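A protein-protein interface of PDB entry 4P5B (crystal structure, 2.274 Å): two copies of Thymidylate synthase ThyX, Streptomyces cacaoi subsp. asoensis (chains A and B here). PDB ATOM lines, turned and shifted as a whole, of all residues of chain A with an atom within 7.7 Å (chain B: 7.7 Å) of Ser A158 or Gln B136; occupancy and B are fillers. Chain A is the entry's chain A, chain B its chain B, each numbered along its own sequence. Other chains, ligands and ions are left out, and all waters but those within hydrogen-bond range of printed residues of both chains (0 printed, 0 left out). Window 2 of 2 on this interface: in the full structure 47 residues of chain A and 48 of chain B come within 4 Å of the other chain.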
ATOM      1  N   GLU A 151       2.181 -18.025  -6.922  1.00  0.00           N
ATOM      2  CA  GLU A 151       2.784 -18.527  -5.710  1.00  0.00           C
ATOM      3  C   GLU A 151       2.646 -20.019  -5.569  1.00  0.00           C
ATOM      4  O   GLU A 151       3.531 -20.653  -5.011  1.00  0.00           O
ATOM      5  CB  GLU A 151       2.151 -17.854  -4.489  1.00  0.00           C
ATOM      6  CG  GLU A 151       2.468 -16.331  -4.364  1.00  0.00           C
ATOM      7  CD  GLU A 151       3.972 -15.980  -4.531  1.00  0.00           C
ATOM      8  OE1 GLU A 151       4.880 -16.786  -4.116  1.00  0.00           O
ATOM      9  OE2 GLU A 151       4.235 -14.902  -5.121  1.00  0.00           O
ATOM     10  N   TYR A 152       1.519 -20.599  -6.018  1.00  0.00           N
ATOM     11  CA  TYR A 152       1.373 -22.039  -5.949  1.00  0.00           C
ATOM     12  C   TYR A 152       2.481 -22.646  -6.834  1.00  0.00           C
ATOM     13  O   TYR A 152       3.236 -23.582  -6.396  1.00  0.00           O
ATOM     14  CB  TYR A 152      -0.034 -22.432  -6.376  1.00  0.00           C
ATOM     15  CG  TYR A 152      -0.302 -23.912  -6.628  1.00  0.00           C
ATOM     16  CD1 TYR A 152      -0.633 -24.368  -7.899  1.00  0.00           C
ATOM     17  CD2 TYR A 152      -0.265 -24.826  -5.597  1.00  0.00           C
ATOM     18  CE1 TYR A 152      -0.930 -25.725  -8.151  1.00  0.00           C
ATOM     19  CE2 TYR A 152      -0.536 -26.150  -5.805  1.00  0.00           C
ATOM     20  CZ  TYR A 152      -0.883 -26.605  -7.083  1.00  0.00           C
ATOM     21  OH  TYR A 152      -1.147 -27.933  -7.270  1.00  0.00           O
ATOM     22  N   GLN A 153       2.660 -22.069  -8.028  1.00  0.00           N
ATOM     23  CA  GLN A 153       3.716 -22.564  -8.928  1.00  0.00           C
ATOM     24  C   GLN A 153       5.138 -22.408  -8.359  1.00  0.00           C
ATOM     25  O   GLN A 153       5.976 -23.345  -8.478  1.00  0.00           O
ATOM     26  CB  GLN A 153       3.615 -21.985 -10.349  1.00  0.00           C
ATOM     27  CG  GLN A 153       2.534 -22.571 -11.218  1.00  0.00           C
ATOM     28  CD  GLN A 153       2.664 -24.086 -11.371  1.00  0.00           C
ATOM     29  OE1 GLN A 153       3.751 -24.603 -11.678  1.00  0.00           O
ATOM     30  NE2 GLN A 153       1.557 -24.813 -11.149  1.00  0.00           N
ATOM     31  N   ARG A 154       5.409 -21.262  -7.748  1.00  0.00           N
ATOM     32  CA  ARG A 154       6.715 -21.034  -7.146  1.00  0.00           C
ATOM     33  C   ARG A 154       7.009 -21.993  -5.971  1.00  0.00           C
ATOM     34  O   ARG A 154       8.129 -22.505  -5.861  1.00  0.00           O
ATOM     35  CB  ARG A 154       6.931 -19.561  -6.759  1.00  0.00           C
ATOM     36  CG  ARG A 154       7.869 -19.416  -5.523  1.00  0.00           C
ATOM     37  CD  ARG A 154       8.658 -18.083  -5.437  1.00  0.00           C
ATOM     38  NE  ARG A 154       7.764 -16.921  -5.335  1.00  0.00           N
ATOM     39  CZ  ARG A 154       7.502 -16.077  -6.336  1.00  0.00           C
ATOM     40  NH1 ARG A 154       6.667 -15.058  -6.142  1.00  0.00           N
ATOM     41  NH2 ARG A 154       8.075 -16.249  -7.529  1.00  0.00           N
ATOM     42  N   LEU A 155       6.003 -22.317  -5.147  1.00  0.00           N
ATOM     43  CA  LEU A 155       6.188 -23.334  -4.109  1.00  0.00           C
ATOM     44  C   LEU A 155       6.481 -24.715  -4.688  1.00  0.00           C
ATOM     45  O   LEU A 155       7.415 -25.362  -4.241  1.00  0.00           O
ATOM     46  CB  LEU A 155       5.002 -23.393  -3.169  1.00  0.00           C
ATOM     47  CG  LEU A 155       4.825 -22.074  -2.414  1.00  0.00           C
ATOM     48  CD1 LEU A 155       3.597 -22.069  -1.579  1.00  0.00           C
ATOM     49  CD2 LEU A 155       6.051 -21.684  -1.536  1.00  0.00           C
ATOM     50  N   LEU A 156       5.716 -25.160  -5.685  1.00  0.00           N
ATOM     51  CA  LEU A 156       6.029 -26.432  -6.356  1.00  0.00           C
ATOM     52  C   LEU A 156       7.461 -26.443  -6.925  1.00  0.00           C
ATOM     53  O   LEU A 156       8.245 -27.387  -6.697  1.00  0.00           O
ATOM     54  CB  LEU A 156       5.034 -26.745  -7.487  1.00  0.00           C
ATOM     55  CG  LEU A 156       3.596 -26.977  -7.032  1.00  0.00           C
ATOM     56  CD1 LEU A 156       2.567 -26.863  -8.195  1.00  0.00           C
ATOM     57  CD2 LEU A 156       3.465 -28.302  -6.189  1.00  0.00           C
ATOM     58  N   ASP A 157       7.772 -25.371  -7.662  1.00  0.00           N
ATOM     59  CA  ASP A 157       9.067 -25.193  -8.313  1.00  0.00           C
ATOM     60  C   ASP A 157      10.213 -25.149  -7.280  1.00  0.00           C
ATOM     61  O   ASP A 157      11.384 -25.330  -7.665  1.00  0.00           O
ATOM     62  CB  ASP A 157       9.083 -23.918  -9.180  1.00  0.00           C
ATOM     63  CG  ASP A 157       8.299 -24.077 -10.519  1.00  0.00           C
ATOM     64  OD1 ASP A 157       7.738 -25.172 -10.790  1.00  0.00           O
ATOM     65  OD2 ASP A 157       8.245 -23.097 -11.312  1.00  0.00           O
ATOM     66  N   SER A 158       9.914 -24.926  -5.995  1.00  0.00           N
ATOM     67  CA  SER A 158      10.977 -25.009  -4.988  1.00  0.00           C
ATOM     68  C   SER A 158      11.042 -26.346  -4.312  1.00  0.00           C
ATOM     69  O   SER A 158      11.752 -26.447  -3.322  1.00  0.00           O
ATOM     70  CB  SER A 158      10.757 -24.004  -3.871  1.00  0.00           C
ATOM     71  OG  SER A 158      10.179 -22.822  -4.376  1.00  0.00           O
ATOM     72  N   GLY A 159      10.238 -27.324  -4.770  1.00  0.00           N
ATOM     73  CA  GLY A 159      10.136 -28.656  -4.149  1.00  0.00           C
ATOM     74  C   GLY A 159       9.219 -28.768  -2.916  1.00  0.00           C
ATOM     75  O   GLY A 159       9.308 -29.748  -2.146  1.00  0.00           O
ATOM     76  N   ILE A 160       8.341 -27.771  -2.698  1.00  0.00           N
ATOM     77  CA  ILE A 160       7.329 -27.865  -1.642  1.00  0.00           C
ATOM     78  C   ILE A 160       6.235 -28.900  -2.071  1.00  0.00           C
ATOM     79  O   ILE A 160       5.826 -28.971  -3.256  1.00  0.00           O
ATOM     80  CB  ILE A 160       6.706 -26.481  -1.313  1.00  0.00           C
ATOM     81  CG1 ILE A 160       7.810 -25.472  -0.922  1.00  0.00           C
ATOM     82  CG2 ILE A 160       5.561 -26.587  -0.234  1.00  0.00           C
ATOM     83  CD1 ILE A 160       8.709 -26.018   0.115  1.00  0.00           C
ATOM     84  N   ALA A 161       5.865 -29.755  -1.128  1.00  0.00           N
ATOM     85  CA  ALA A 161       4.910 -30.812  -1.379  1.00  0.00           C
ATOM     86  C   ALA A 161       3.556 -30.222  -1.878  1.00  0.00           C
ATOM     87  O   ALA A 161       3.120 -29.120  -1.477  1.00  0.00           O
ATOM     88  CB  ALA A 161       4.693 -31.616  -0.110  1.00  0.00           C
ATOM     89  N   GLN B 117       6.576 -33.476   4.863  1.00  0.00           N
ATOM     90  CA  GLN B 117       5.656 -33.211   3.739  1.00  0.00           C
ATOM     91  C   GLN B 117       5.471 -34.513   2.974  1.00  0.00           C
ATOM     92  O   GLN B 117       6.440 -35.241   2.791  1.00  0.00           O
ATOM     93  CB  GLN B 117       6.232 -32.143   2.809  1.00  0.00           C
ATOM     94  CG  GLN B 117       6.410 -30.756   3.419  1.00  0.00           C
ATOM     95  CD  GLN B 117       7.467 -29.922   2.673  1.00  0.00           C
ATOM     96  OE1 GLN B 117       8.477 -29.561   3.238  1.00  0.00           O
ATOM     97  NE2 GLN B 117       7.225 -29.638   1.400  1.00  0.00           N
ATOM     98  N   THR B 131      14.087 -26.816   6.357  1.00  0.00           N
ATOM     99  CA  THR B 131      13.606 -25.506   6.815  1.00  0.00           C
ATOM    100  C   THR B 131      14.235 -24.285   6.150  1.00  0.00           C
ATOM    101  O   THR B 131      14.268 -23.193   6.732  1.00  0.00           O
ATOM    102  CB  THR B 131      13.689 -25.393   8.378  1.00  0.00           C
ATOM    103  OG1 THR B 131      13.173 -26.593   8.995  1.00  0.00           O
ATOM    104  CG2 THR B 131      12.914 -24.153   8.917  1.00  0.00           C
ATOM    105  N   ASP B 132      14.713 -24.433   4.920  1.00  0.00           N
ATOM    106  CA  ASP B 132      14.795 -23.225   4.078  1.00  0.00           C
ATOM    107  C   ASP B 132      13.401 -22.936   3.430  1.00  0.00           C
ATOM    108  O   ASP B 132      13.091 -21.811   2.981  1.00  0.00           O
ATOM    109  CB  ASP B 132      15.919 -23.359   3.041  1.00  0.00           C
ATOM    110  CG  ASP B 132      16.634 -22.033   2.789  1.00  0.00           C
ATOM    111  OD1 ASP B 132      16.198 -21.012   3.388  1.00  0.00           O
ATOM    112  OD2 ASP B 132      17.627 -22.022   2.007  1.00  0.00           O
ATOM    113  N   ASP B 133      12.579 -23.991   3.441  1.00  0.00           N
ATOM    114  CA  ASP B 133      11.255 -24.042   2.857  1.00  0.00           C
ATOM    115  C   ASP B 133      10.310 -23.118   3.584  1.00  0.00           C
ATOM    116  O   ASP B 133       9.481 -22.439   2.976  1.00  0.00           O
ATOM    117  CB  ASP B 133      10.707 -25.469   2.964  1.00  0.00           C
ATOM    118  CG  ASP B 133      11.531 -26.486   2.171  1.00  0.00           C
ATOM    119  OD1 ASP B 133      12.473 -26.061   1.456  1.00  0.00           O
ATOM    120  OD2 ASP B 133      11.239 -27.709   2.267  1.00  0.00           O
ATOM    121  N   HIS B 134      10.443 -23.116   4.901  1.00  0.00           N
ATOM    122  CA  HIS B 134       9.513 -22.432   5.770  1.00  0.00           C
ATOM    123  C   HIS B 134       9.462 -20.949   5.450  1.00  0.00           C
ATOM    124  O   HIS B 134       8.373 -20.349   5.462  1.00  0.00           O
ATOM    125  CB  HIS B 134       9.862 -22.672   7.243  1.00  0.00           C
ATOM    126  CG  HIS B 134       8.954 -21.964   8.199  1.00  0.00           C
ATOM    127  ND1 HIS B 134       7.700 -22.438   8.525  1.00  0.00           N
ATOM    128  CD2 HIS B 134       9.108 -20.808   8.883  1.00  0.00           C
ATOM    129  CE1 HIS B 134       7.131 -21.618   9.392  1.00  0.00           C
ATOM    130  NE2 HIS B 134       7.965 -20.620   9.620  1.00  0.00           N
ATOM    131  N   GLN B 135      10.620 -20.362   5.144  1.00  0.00           N
ATOM    132  CA  GLN B 135      10.644 -18.946   4.897  1.00  0.00           C
ATOM    133  C   GLN B 135      10.034 -18.717   3.548  1.00  0.00           C
ATOM    134  O   GLN B 135       9.267 -17.773   3.375  1.00  0.00           O
ATOM    135  CB  GLN B 135      12.054 -18.378   4.934  1.00  0.00           C
ATOM    136  CG  GLN B 135      12.159 -17.111   5.750  1.00  0.00           C
ATOM    137  CD  GLN B 135      12.495 -17.419   7.216  1.00  0.00           C
ATOM    138  OE1 GLN B 135      11.868 -18.306   7.839  1.00  0.00           O
ATOM    139  NE2 GLN B 135      13.498 -16.706   7.771  1.00  0.00           N
ATOM    140  N   GLN B 136      10.371 -19.590   2.601  1.00  0.00           N
ATOM    141  CA  GLN B 136       9.822 -19.478   1.254  1.00  0.00           C
ATOM    142  C   GLN B 136       8.285 -19.588   1.311  1.00  0.00           C
ATOM    143  O   GLN B 136       7.582 -18.747   0.728  1.00  0.00           O
ATOM    144  CB  GLN B 136      10.479 -20.490   0.292  1.00  0.00           C
ATOM    145  CG  GLN B 136       9.822 -20.602  -1.099  1.00  0.00           C
ATOM    146  CD  GLN B 136       9.691 -19.252  -1.808  1.00  0.00           C
ATOM    147  OE1 GLN B 136       8.568 -18.767  -2.080  1.00  0.00           O
ATOM    148  NE2 GLN B 136      10.844 -18.621  -2.104  1.00  0.00           N
ATOM    149  N   VAL B 137       7.783 -20.578   2.070  1.00  0.00           N
ATOM    150  CA  VAL B 137       6.310 -20.764   2.254  1.00  0.00           C
ATOM    151  C   VAL B 137       5.670 -19.541   2.964  1.00  0.00           C
ATOM    152  O   VAL B 137       4.639 -19.018   2.525  1.00  0.00           O
ATOM    153  CB  VAL B 137       5.980 -22.085   3.005  1.00  0.00           C
ATOM    154  CG1 VAL B 137       4.555 -22.081   3.492  1.00  0.00           C
ATOM    155  CG2 VAL B 137       6.267 -23.288   2.129  1.00  0.00           C
ATOM    156  N   VAL B 138       6.310 -19.064   4.031  1.00  0.00           N
ATOM    157  CA  VAL B 138       5.793 -17.878   4.718  1.00  0.00           C
ATOM    158  C   VAL B 138       5.753 -16.682   3.762  1.00  0.00           C
ATOM    159  O   VAL B 138       4.743 -15.968   3.681  1.00  0.00           O
ATOM    160  CB  VAL B 138       6.605 -17.520   5.987  1.00  0.00           C
ATOM    161  CG1 VAL B 138       6.396 -16.048   6.394  1.00  0.00           C
ATOM    162  CG2 VAL B 138       6.261 -18.449   7.099  1.00  0.00           C
ATOM    163  N   ARG B 139       6.838 -16.484   3.031  1.00  0.00           N
ATOM    164  CA  ARG B 139       6.913 -15.405   2.050  1.00  0.00           C
ATOM    165  C   ARG B 139       5.831 -15.556   0.953  1.00  0.00           C
ATOM    166  O   ARG B 139       5.123 -14.597   0.683  1.00  0.00           O
ATOM    167  CB  ARG B 139       8.309 -15.365   1.448  1.00  0.00           C
ATOM    168  CG  ARG B 139       8.772 -13.997   0.891  1.00  0.00           C
ATOM    169  CD  ARG B 139      10.337 -13.856   0.840  1.00  0.00           C
ATOM    170  NE  ARG B 139      10.997 -14.999   0.186  1.00  0.00           N
ATOM    171  CZ  ARG B 139      11.839 -15.874   0.773  1.00  0.00           C
ATOM    172  NH1 ARG B 139      12.191 -15.755   2.060  1.00  0.00           N
ATOM    173  NH2 ARG B 139      12.356 -16.879   0.053  1.00  0.00           N
ATOM    174  N   SER B 140       5.659 -16.746   0.356  1.00  0.00           N
ATOM    175  CA  SER B 140       4.592 -16.932  -0.658  1.00  0.00           C
ATOM    176  C   SER B 140       3.188 -16.735  -0.121  1.00  0.00           C
ATOM    177  O   SER B 140       2.331 -16.026  -0.715  1.00  0.00           O
ATOM    178  CB  SER B 140       4.693 -18.290  -1.334  1.00  0.00           C
ATOM    179  OG  SER B 140       5.758 -18.268  -2.247  1.00  0.00           O
ATOM    180  N   ALA B 141       2.959 -17.376   1.013  1.00  0.00           N
ATOM    181  CA  ALA B 141       1.688 -17.267   1.690  1.00  0.00           C
ATOM    182  C   ALA B 141       1.361 -15.793   1.960  1.00  0.00           C
ATOM    183  O   ALA B 141       0.246 -15.327   1.649  1.00  0.00           O
ATOM    184  CB  ALA B 141       1.720 -18.058   2.977  1.00  0.00           C
ATOM    185  N   THR B 142       2.320 -15.049   2.517  1.00  0.00           N
ATOM    186  CA  THR B 142       2.008 -13.669   2.946  1.00  0.00           C
ATOM    187  C   THR B 142       1.563 -12.863   1.762  1.00  0.00           C
ATOM    188  O   THR B 142       0.627 -12.096   1.848  1.00  0.00           O
ATOM    189  CB  THR B 142       3.172 -12.959   3.686  1.00  0.00           C
ATOM    190  OG1 THR B 142       3.439 -13.664   4.894  1.00  0.00           O
ATOM    191  CG2 THR B 142       2.809 -11.544   4.088  1.00  0.00           C
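The side-chain hydroxyl (OG) of Ser B140 sits at hydrogen-bond distance from the side-chain carboxylate (OE1) of Glu A151 (2.5 Å).
The backbone NH of Ala A161 sits close to the side-chain amide nitrogen of Gln B117 (2.9 Å).
Arg A154 touches Gln B136 (CD to OE1, 3.4 Å).
Arg A154 touches Ser B140.
Gln B136 touches Leu A155 (OE1 to CD2, 3.9 Å).
Leu A155 touches Val B137.
Leu A155 touches Ser B140 (CD2 to OG, 3.5 Å).
OG of Ser A158 touches CG of Gln B136, at 3.97 Å.
Gln B117 touches Ile A160 (NE2 to CA, 3.5 Å).
CD1 of Ile A160 touches CG of Asp B133, at 3.5 Å.
Of the 13 printed residues of chain B, 5 touch a printed residue of chain A.
Printed residues of chain B that touch a printed residue of chain A: Gln B117, Asp B133, Gln B136, Val B137 and Ser B140.
Hydrophobic or aromatic side chains of chain A that line the printed part of chain B: Leu A155, Ile A160 and Ala A161.
NH2 of Arg B139 lies close to NE2 of Gln B136, at 3.2 Å.
OG of Ser A158 sits at hydrogen-bond distance from O of Arg A154, at 2.6 Å.
OG of Ser B140 is in hydrogen-bond range of OE1 of Gln B136, at 2.9 Å.
OE2 of Glu A151 lies within salt-bridge range of NH1 of Arg A154 (2.6 Å).
O of Leu A155 sits at hydrogen-bond distance from N of Ile A160 (3.0 Å).
The side-chain carboxylate of Asp B133 sits close to the side-chain amide oxygen of Gln B117.
Of the printed residues of chain B, Glu A151 touches Ser B140 (2.5 Å).
Of the printed residues of chain B, Arg A154 touches Gln B136 (3.4 Å) and Ser B140 (3.9 Å).
Ser A158 touches just one residue of chain B: Gln B136.
Of the printed residues of chain B, Ala A161 touches Gln B117.
Of the printed residues of chain A, Gln B117 touches Ile A160 (3.5 Å) and Ala A161 (2.9 Å).
His B134 touches none of the printed residues of chain A.
Gln B136 touches three residues of chain A.
Printed residues of chain A within 4 Å of Ser B140: Glu A151, Arg A154 and Leu A155.
Thr B142 touches none of the printed residues of chain A.
The nearest residue of chain B that does not touch Ser A158 is Asp B133 (4.8 Å).
The nearest printed residue of chain A that does not touch Ser B140 is Tyr A152 (6.1 Å).
No position is printed for both chains.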
